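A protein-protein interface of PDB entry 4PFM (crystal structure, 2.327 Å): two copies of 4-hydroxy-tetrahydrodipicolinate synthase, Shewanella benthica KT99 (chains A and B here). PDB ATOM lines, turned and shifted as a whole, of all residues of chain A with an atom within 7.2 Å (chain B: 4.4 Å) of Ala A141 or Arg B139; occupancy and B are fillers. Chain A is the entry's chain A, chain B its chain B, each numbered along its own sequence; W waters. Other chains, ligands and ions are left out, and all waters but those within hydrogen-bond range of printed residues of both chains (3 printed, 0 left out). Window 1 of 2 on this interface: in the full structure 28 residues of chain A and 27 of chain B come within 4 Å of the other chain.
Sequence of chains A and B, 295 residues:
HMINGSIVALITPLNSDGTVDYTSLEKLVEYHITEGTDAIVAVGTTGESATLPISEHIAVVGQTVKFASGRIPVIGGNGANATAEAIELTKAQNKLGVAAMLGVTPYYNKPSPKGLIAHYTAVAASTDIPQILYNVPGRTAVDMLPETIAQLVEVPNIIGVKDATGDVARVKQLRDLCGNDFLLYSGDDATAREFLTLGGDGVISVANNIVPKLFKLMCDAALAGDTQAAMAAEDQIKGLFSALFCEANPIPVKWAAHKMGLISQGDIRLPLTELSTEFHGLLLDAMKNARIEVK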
ATOM      1  N   THR A 105       9.065  19.292   6.512  1.00  0.00           N
ATOM      2  CA  THR A 105      10.114  19.749   5.613  1.00  0.00           C
ATOM      3  C   THR A 105      10.195  18.859   4.381  1.00  0.00           C
ATOM      4  O   THR A 105      10.012  17.616   4.511  1.00  0.00           O
ATOM      5  CB  THR A 105      11.540  19.580   6.299  1.00  0.00           C
ATOM      6  OG1 THR A 105      11.742  18.170   6.610  1.00  0.00           O
ATOM      7  CG2 THR A 105      11.642  20.421   7.565  1.00  0.00           C
ATOM      8  N   PRO A 106      10.557  19.430   3.210  1.00  0.00           N
ATOM      9  CA  PRO A 106      10.894  18.657   2.064  1.00  0.00           C
ATOM     10  C   PRO A 106      11.744  17.412   2.317  1.00  0.00           C
ATOM     11  O   PRO A 106      12.816  17.501   2.882  1.00  0.00           O
ATOM     12  CB  PRO A 106      11.692  19.653   1.206  1.00  0.00           C
ATOM     13  CG  PRO A 106      11.001  20.997   1.509  1.00  0.00           C
ATOM     14  CD  PRO A 106      10.820  20.872   2.996  1.00  0.00           C
ATOM     15  N   TYR A 107      11.280  16.252   1.820  1.00  0.00           N
ATOM     16  CA  TYR A 107      11.951  15.000   1.975  1.00  0.00           C
ATOM     17  C   TYR A 107      12.660  14.640   0.709  1.00  0.00           C
ATOM     18  O   TYR A 107      12.269  15.052  -0.380  1.00  0.00           O
ATOM     19  CB  TYR A 107      10.896  13.917   2.306  1.00  0.00           C
ATOM     20  CG  TYR A 107       9.578  14.139   1.664  1.00  0.00           C
ATOM     21  CD1 TYR A 107       8.615  14.909   2.305  1.00  0.00           C
ATOM     22  CD2 TYR A 107       9.286  13.622   0.420  1.00  0.00           C
ATOM     23  CE1 TYR A 107       7.358  15.178   1.699  1.00  0.00           C
ATOM     24  CE2 TYR A 107       8.031  13.854  -0.208  1.00  0.00           C
ATOM     25  CZ  TYR A 107       7.077  14.637   0.455  1.00  0.00           C
ATOM     26  OH  TYR A 107       5.831  14.935  -0.101  1.00  0.00           O
ATOM     27  N   TYR A 108      13.684  13.818   0.831  1.00  0.00           N
ATOM     28  CA  TYR A 108      14.327  13.168  -0.320  1.00  0.00           C
ATOM     29  C   TYR A 108      15.258  14.076  -1.140  1.00  0.00           C
ATOM     30  O   TYR A 108      16.352  13.636  -1.487  1.00  0.00           O
ATOM     31  CB  TYR A 108      13.301  12.472  -1.251  1.00  0.00           C
ATOM     32  CG  TYR A 108      13.911  11.963  -2.538  1.00  0.00           C
ATOM     33  CD1 TYR A 108      14.679  10.776  -2.545  1.00  0.00           C
ATOM     34  CD2 TYR A 108      13.734  12.667  -3.762  1.00  0.00           C
ATOM     35  CE1 TYR A 108      15.268  10.309  -3.683  1.00  0.00           C
ATOM     36  CE2 TYR A 108      14.312  12.181  -4.955  1.00  0.00           C
ATOM     37  CZ  TYR A 108      15.071  11.000  -4.883  1.00  0.00           C
ATOM     38  OH  TYR A 108      15.656  10.492  -6.024  1.00  0.00           O
ATOM     39  N   ASN A 109      14.858  15.326  -1.425  1.00  0.00           N
ATOM     40  CA  ASN A 109      15.731  16.210  -2.232  1.00  0.00           C
ATOM     41  C   ASN A 109      16.715  17.082  -1.401  1.00  0.00           C
ATOM     42  O   ASN A 109      17.593  17.724  -1.980  1.00  0.00           O
ATOM     43  CB  ASN A 109      14.979  17.063  -3.278  1.00  0.00           C
ATOM     44  CG  ASN A 109      13.913  17.971  -2.673  1.00  0.00           C
ATOM     45  OD1 ASN A 109      13.625  17.903  -1.451  1.00  0.00           O
ATOM     46  ND2 ASN A 109      13.231  18.756  -3.541  1.00  0.00           N
ATOM     47  N   LYS A 110      16.653  17.024  -0.074  1.00  0.00           N
ATOM     48  CA  LYS A 110      17.726  17.594   0.767  1.00  0.00           C
ATOM     49  C   LYS A 110      18.055  19.126   0.559  1.00  0.00           C
ATOM     50  O   LYS A 110      19.184  19.477   0.240  1.00  0.00           O
ATOM     51  CB  LYS A 110      19.029  16.788   0.607  1.00  0.00           C
ATOM     52  CG  LYS A 110      19.125  15.490   1.384  1.00  0.00           C
ATOM     53  CD  LYS A 110      20.624  15.035   1.599  1.00  0.00           C
ATOM     54  CE  LYS A 110      21.137  15.675   2.924  1.00  0.00           C
ATOM     55  NZ  LYS A 110      22.538  15.335   3.406  1.00  0.00           N
ATOM     56  N   PRO A 111      17.076  20.024   0.751  1.00  0.00           N
ATOM     57  CA  PRO A 111      17.388  21.436   0.576  1.00  0.00           C
ATOM     58  C   PRO A 111      18.348  21.977   1.665  1.00  0.00           C
ATOM     59  O   PRO A 111      18.425  21.438   2.777  1.00  0.00           O
ATOM     60  CB  PRO A 111      16.016  22.099   0.681  1.00  0.00           C
ATOM     61  CG  PRO A 111      15.300  21.204   1.591  1.00  0.00           C
ATOM     62  CD  PRO A 111      15.704  19.826   1.234  1.00  0.00           C
ATOM     63  N   VAL A 136      11.451  15.829  10.748  1.00  0.00           N
ATOM     64  CA  VAL A 136      11.595  14.363  11.015  1.00  0.00           C
ATOM     65  C   VAL A 136      12.712  13.794  10.130  1.00  0.00           C
ATOM     66  O   VAL A 136      12.418  13.209   9.089  1.00  0.00           O
ATOM     67  CB  VAL A 136      10.215  13.615  10.890  1.00  0.00           C
ATOM     68  CG1 VAL A 136       9.493  13.876   9.527  1.00  0.00           C
ATOM     69  CG2 VAL A 136      10.354  12.104  11.219  1.00  0.00           C
ATOM     70  N   PRO A 137      13.996  14.063  10.486  1.00  0.00           N
ATOM     71  CA  PRO A 137      15.098  13.695   9.555  1.00  0.00           C
ATOM     72  C   PRO A 137      15.243  12.187   9.357  1.00  0.00           C
ATOM     73  O   PRO A 137      15.778  11.733   8.325  1.00  0.00           O
ATOM     74  CB  PRO A 137      16.361  14.208  10.268  1.00  0.00           C
ATOM     75  CG  PRO A 137      16.002  14.367  11.670  1.00  0.00           C
ATOM     76  CD  PRO A 137      14.524  14.831  11.645  1.00  0.00           C
ATOM     77  N   GLY A 138      14.727  11.440  10.317  1.00  0.00           N
ATOM     78  CA  GLY A 138      14.658   9.995  10.206  1.00  0.00           C
ATOM     79  C   GLY A 138      13.819   9.562   9.028  1.00  0.00           C
ATOM     80  O   GLY A 138      14.005   8.447   8.577  1.00  0.00           O
ATOM     81  N   ARG A 139      12.927  10.422   8.494  1.00  0.00           N
ATOM     82  CA  ARG A 139      12.211  10.092   7.240  1.00  0.00           C
ATOM     83  C   ARG A 139      12.589  10.964   6.069  1.00  0.00           C
ATOM     84  O   ARG A 139      12.432  10.509   4.910  1.00  0.00           O
ATOM     85  CB  ARG A 139      10.702  10.187   7.372  1.00  0.00           C
ATOM     86  CG  ARG A 139      10.102   9.211   8.310  1.00  0.00           C
ATOM     87  CD  ARG A 139       8.644   9.600   8.595  1.00  0.00           C
ATOM     88  NE  ARG A 139       7.944   8.483   9.276  1.00  0.00           N
ATOM     89  CZ  ARG A 139       7.419   7.409   8.647  1.00  0.00           C
ATOM     90  NH1 ARG A 139       7.453   7.310   7.310  1.00  0.00           N
ATOM     91  NH2 ARG A 139       6.784   6.480   9.345  1.00  0.00           N
ATOM     92  N   THR A 140      13.040  12.196   6.315  1.00  0.00           N
ATOM     93  CA  THR A 140      13.160  13.143   5.203  1.00  0.00           C
ATOM     94  C   THR A 140      14.579  13.248   4.749  1.00  0.00           C
ATOM     95  O   THR A 140      14.848  13.703   3.653  1.00  0.00           O
ATOM     96  CB  THR A 140      12.767  14.576   5.582  1.00  0.00           C
ATOM     97  OG1 THR A 140      13.642  15.030   6.647  1.00  0.00           O
ATOM     98  CG2 THR A 140      11.321  14.614   6.048  1.00  0.00           C
ATOM     99  N   ALA A 141      15.506  12.801   5.579  1.00  0.00           N
ATOM    100  CA  ALA A 141      16.936  12.995   5.284  1.00  0.00           C
ATOM    101  C   ALA A 141      17.442  14.459   5.395  1.00  0.00           C
ATOM    102  O   ALA A 141      18.531  14.748   4.872  1.00  0.00           O
ATOM    103  CB  ALA A 141      17.294  12.416   3.956  1.00  0.00           C
ATOM    104  N   VAL A 142      16.665  15.380   6.018  1.00  0.00           N
ATOM    105  CA  VAL A 142      17.220  16.703   6.447  1.00  0.00           C
ATOM    106  C   VAL A 142      16.854  16.984   7.867  1.00  0.00           C
ATOM    107  O   VAL A 142      15.687  16.894   8.235  1.00  0.00           O
ATOM    108  CB  VAL A 142      16.705  17.975   5.713  1.00  0.00           C
ATOM    109  CG1 VAL A 142      17.532  18.310   4.627  1.00  0.00           C
ATOM    110  CG2 VAL A 142      15.180  17.856   5.306  1.00  0.00           C
ATOM    111  N   ASP A 143      17.842  17.438   8.636  1.00  0.00           N
ATOM    112  CA  ASP A 143      17.579  17.841   9.999  1.00  0.00           C
ATOM    113  C   ASP A 143      17.468  19.395   9.987  1.00  0.00           C
ATOM    114  O   ASP A 143      18.471  20.103   9.750  1.00  0.00           O
ATOM    115  CB  ASP A 143      18.680  17.310  10.922  1.00  0.00           C
ATOM    116  CG  ASP A 143      18.296  17.348  12.370  1.00  0.00           C
ATOM    117  OD1 ASP A 143      17.189  17.858  12.735  1.00  0.00           O
ATOM    118  OD2 ASP A 143      19.118  16.849  13.184  1.00  0.00           O
ATOM    119  N   THR B  45      17.307  11.882  -9.810  1.00  0.00           N
ATOM    120  CA  THR B  45      17.478  12.785  -8.699  1.00  0.00           C
ATOM    121  C   THR B  45      18.245  14.034  -9.147  1.00  0.00           C
ATOM    122  O   THR B  45      17.880  15.154  -8.766  1.00  0.00           O
ATOM    123  CB  THR B  45      18.296  12.111  -7.606  1.00  0.00           C
ATOM    124  OG1 THR B  45      17.696  10.848  -7.256  1.00  0.00           O
ATOM    125  CG2 THR B  45      18.332  12.942  -6.397  1.00  0.00           C
ATOM    126  N   VAL B 136      19.114   4.442  -2.764  1.00  0.00           N
ATOM    127  CA  VAL B 136      19.879   5.603  -2.192  1.00  0.00           C
ATOM    128  C   VAL B 136      19.301   5.954  -0.800  1.00  0.00           C
ATOM    129  O   VAL B 136      18.553   6.930  -0.625  1.00  0.00           O
ATOM    130  CB  VAL B 136      19.982   6.866  -3.173  1.00  0.00           C
ATOM    131  CG1 VAL B 136      18.586   7.311  -3.725  1.00  0.00           C
ATOM    132  CG2 VAL B 136      20.727   8.048  -2.527  1.00  0.00           C
ATOM    133  N   PRO B 137      19.650   5.129   0.191  1.00  0.00           N
ATOM    134  CA  PRO B 137      19.184   5.223   1.570  1.00  0.00           C
ATOM    135  C   PRO B 137      19.494   6.574   2.169  1.00  0.00           C
ATOM    136  O   PRO B 137      18.700   7.085   2.972  1.00  0.00           O
ATOM    137  CB  PRO B 137      19.976   4.117   2.306  1.00  0.00           C
ATOM    138  CG  PRO B 137      20.701   3.329   1.238  1.00  0.00           C
ATOM    139  CD  PRO B 137      20.553   3.977  -0.052  1.00  0.00           C
ATOM    140  N   GLY B 138      20.598   7.190   1.749  1.00  0.00           N
ATOM    141  CA  GLY B 138      20.935   8.527   2.253  1.00  0.00           C
ATOM    142  C   GLY B 138      19.839   9.554   1.950  1.00  0.00           C
ATOM    143  O   GLY B 138      19.801  10.606   2.562  1.00  0.00           O
ATOM    144  N   ARG B 139      18.979   9.285   0.980  1.00  0.00           N
ATOM    145  CA  ARG B 139      17.899  10.225   0.598  1.00  0.00           C
ATOM    146  C   ARG B 139      16.510   9.710   0.916  1.00  0.00           C
ATOM    147  O   ARG B 139      15.629  10.516   1.190  1.00  0.00           O
ATOM    148  CB  ARG B 139      17.979  10.576  -0.895  1.00  0.00           C
ATOM    149  CG  ARG B 139      19.155  11.534  -1.230  1.00  0.00           C
ATOM    150  CD  ARG B 139      19.288  11.649  -2.733  1.00  0.00           C
ATOM    151  NE  ARG B 139      20.246  12.719  -3.071  1.00  0.00           N
ATOM    152  CZ  ARG B 139      19.983  14.037  -3.143  1.00  0.00           C
ATOM    153  NH1 ARG B 139      18.739  14.527  -2.942  1.00  0.00           N
ATOM    154  NH2 ARG B 139      20.995  14.869  -3.445  1.00  0.00           N
ATOM    155  N   THR B 140      16.314   8.380   0.906  1.00  0.00           N
ATOM    156  CA  THR B 140      14.988   7.827   0.901  1.00  0.00           C
ATOM    157  C   THR B 140      14.627   7.347   2.272  1.00  0.00           C
ATOM    158  O   THR B 140      13.444   7.149   2.546  1.00  0.00           O
ATOM    159  CB  THR B 140      14.955   6.570  -0.017  1.00  0.00           C
ATOM    160  OG1 THR B 140      15.925   5.629   0.498  1.00  0.00           O
ATOM    161  CG2 THR B 140      15.346   6.959  -1.423  1.00  0.00           C
ATOM    162  N   ALA B 141      15.639   7.183   3.137  1.00  0.00           N
ATOM    163  CA  ALA B 141      15.497   6.561   4.478  1.00  0.00           C
ATOM    164  C   ALA B 141      15.097   5.052   4.473  1.00  0.00           C
ATOM    165  O   ALA B 141      14.718   4.520   5.481  1.00  0.00           O
ATOM    166  CB  ALA B 141      14.556   7.320   5.354  1.00  0.00           C
ATOM    167  N   ALA B 248      23.594  19.595  -1.375  1.00  0.00           N
ATOM    168  CA  ALA B 248      22.916  18.435  -2.001  1.00  0.00           C
ATOM    169  C   ALA B 248      22.912  18.551  -3.512  1.00  0.00           C
ATOM    170  O   ALA B 248      22.590  19.586  -4.098  1.00  0.00           O
ATOM    171  CB  ALA B 248      21.516  18.302  -1.529  1.00  0.00           C
ATOM    172  N   ASN B 249      23.278  17.454  -4.149  1.00  0.00           N
ATOM    173  CA  ASN B 249      23.151  17.335  -5.583  1.00  0.00           C
ATOM    174  C   ASN B 249      21.686  17.436  -5.930  1.00  0.00           C
ATOM    175  O   ASN B 249      20.818  16.896  -5.167  1.00  0.00           O
ATOM    176  CB  ASN B 249      23.742  15.961  -5.959  1.00  0.00           C
ATOM    177  CG  ASN B 249      23.515  15.582  -7.388  1.00  0.00           C
ATOM    178  OD1 ASN B 249      24.044  16.218  -8.307  1.00  0.00           O
ATOM    179  ND2 ASN B 249      22.764  14.472  -7.593  1.00  0.00           N
HETATM  180  O   HOH W   1      18.327  16.948  -4.527  1.00  0.00           O
HETATM  181  O   HOH W   2      21.640  20.943   0.364  1.00  0.00           O
HETATM  182  O   HOH W   3      13.117  10.868   2.239  1.00  0.00           O
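Among the printed residues, pairs that only touch across the chains: Asn A109 with Arg B139 (3.5 Å), Asn A109 with Ala B248 (3.99 Å), Lys A110 with Ala B248 (3.2 Å), Gly A138 with Ala B141 (3.5 Å), Arg A139 with Ala B141 (3.9 Å), Ala A141 with Gly B138 (3.4 Å) and Ala A141 with Arg B139 (3.7 Å).
The backbone carbonyl oxygen (O) of Tyr A107 lies close to the side-chain amide oxygen (OD1) of Asn A109. O of Thr A140 is in hydrogen-bond range of N of Tyr A108. The guanidinium group (NH2) of Arg B139 sits at hydrogen-bond distance from the backbone carbonyl oxygen (O) of Asn B249, at 2.7 Å.
OH of Tyr A108 sits at hydrogen-bond distance from OG1 of Thr B45 (2.4 Å). The guanidinium group of Arg B139 is in hydrogen-bond range of the backbone carbonyl oxygen of Tyr A108, 2.9 Å away.
Of the 9 printed residues of chain B, 5 touch a printed residue of chain A. Hydrophobic or aromatic side chains of chain B within 4 Å of the printed part of chain A: Ala B141 and Ala B248. Of the 15 printed residues of chain A, 6 touch a printed residue of chain B. Among the printed residues, no Asp or Glu carboxylate lies within 4 Å of a Lys or Arg side-chain nitrogen of the other chain.
Water W1 lies within hydrogen-bond range of the backbone carbonyl oxygen of Asn B249, the backbone carbonyl oxygen of Asn A109 and the guanidinium group of Arg B139. Water W3 lies within hydrogen-bond range of the backbone carbonyl oxygen (O) of Arg B139 (2.7 Å), the backbone carbonyl oxygen (O) of Arg A139 (2.8 Å) and the backbone NH (N) of Tyr A108 (3.3 Å). Water W2 bridges the backbone carbonyl oxygen (O) of Lys A110 (2.9 Å) and the backbone NH (N) of Ala B248 (2.9 Å).
Of the printed residues of chain B, Ala A141 touches Gly B138 (3.4 Å) and Arg B139 (3.7 Å). Of chain A, only Ala A141 comes within 4 Å of Gly B138. Of the printed residues of chain A, Thr B45 touches Tyr A108 (2.4 Å). Of the printed residues of chain A, Ala B248 touches Asn A109 (3.99 Å) and Lys A110 (3.2 Å). Of the printed residues of chain B, Lys A110 touches Ala B248. Thr A105 touches none of the printed residues of chain B. The nearest printed residue of chain B that does not touch Ala A141 is Thr B140 (5.2 Å).
Gly A138 touches Ala B141, and with the chains exchanged Ala A141 touches Gly B138. Arg A139 touches Ala B141, and with the chains exchanged Ala A141 touches Arg B139.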
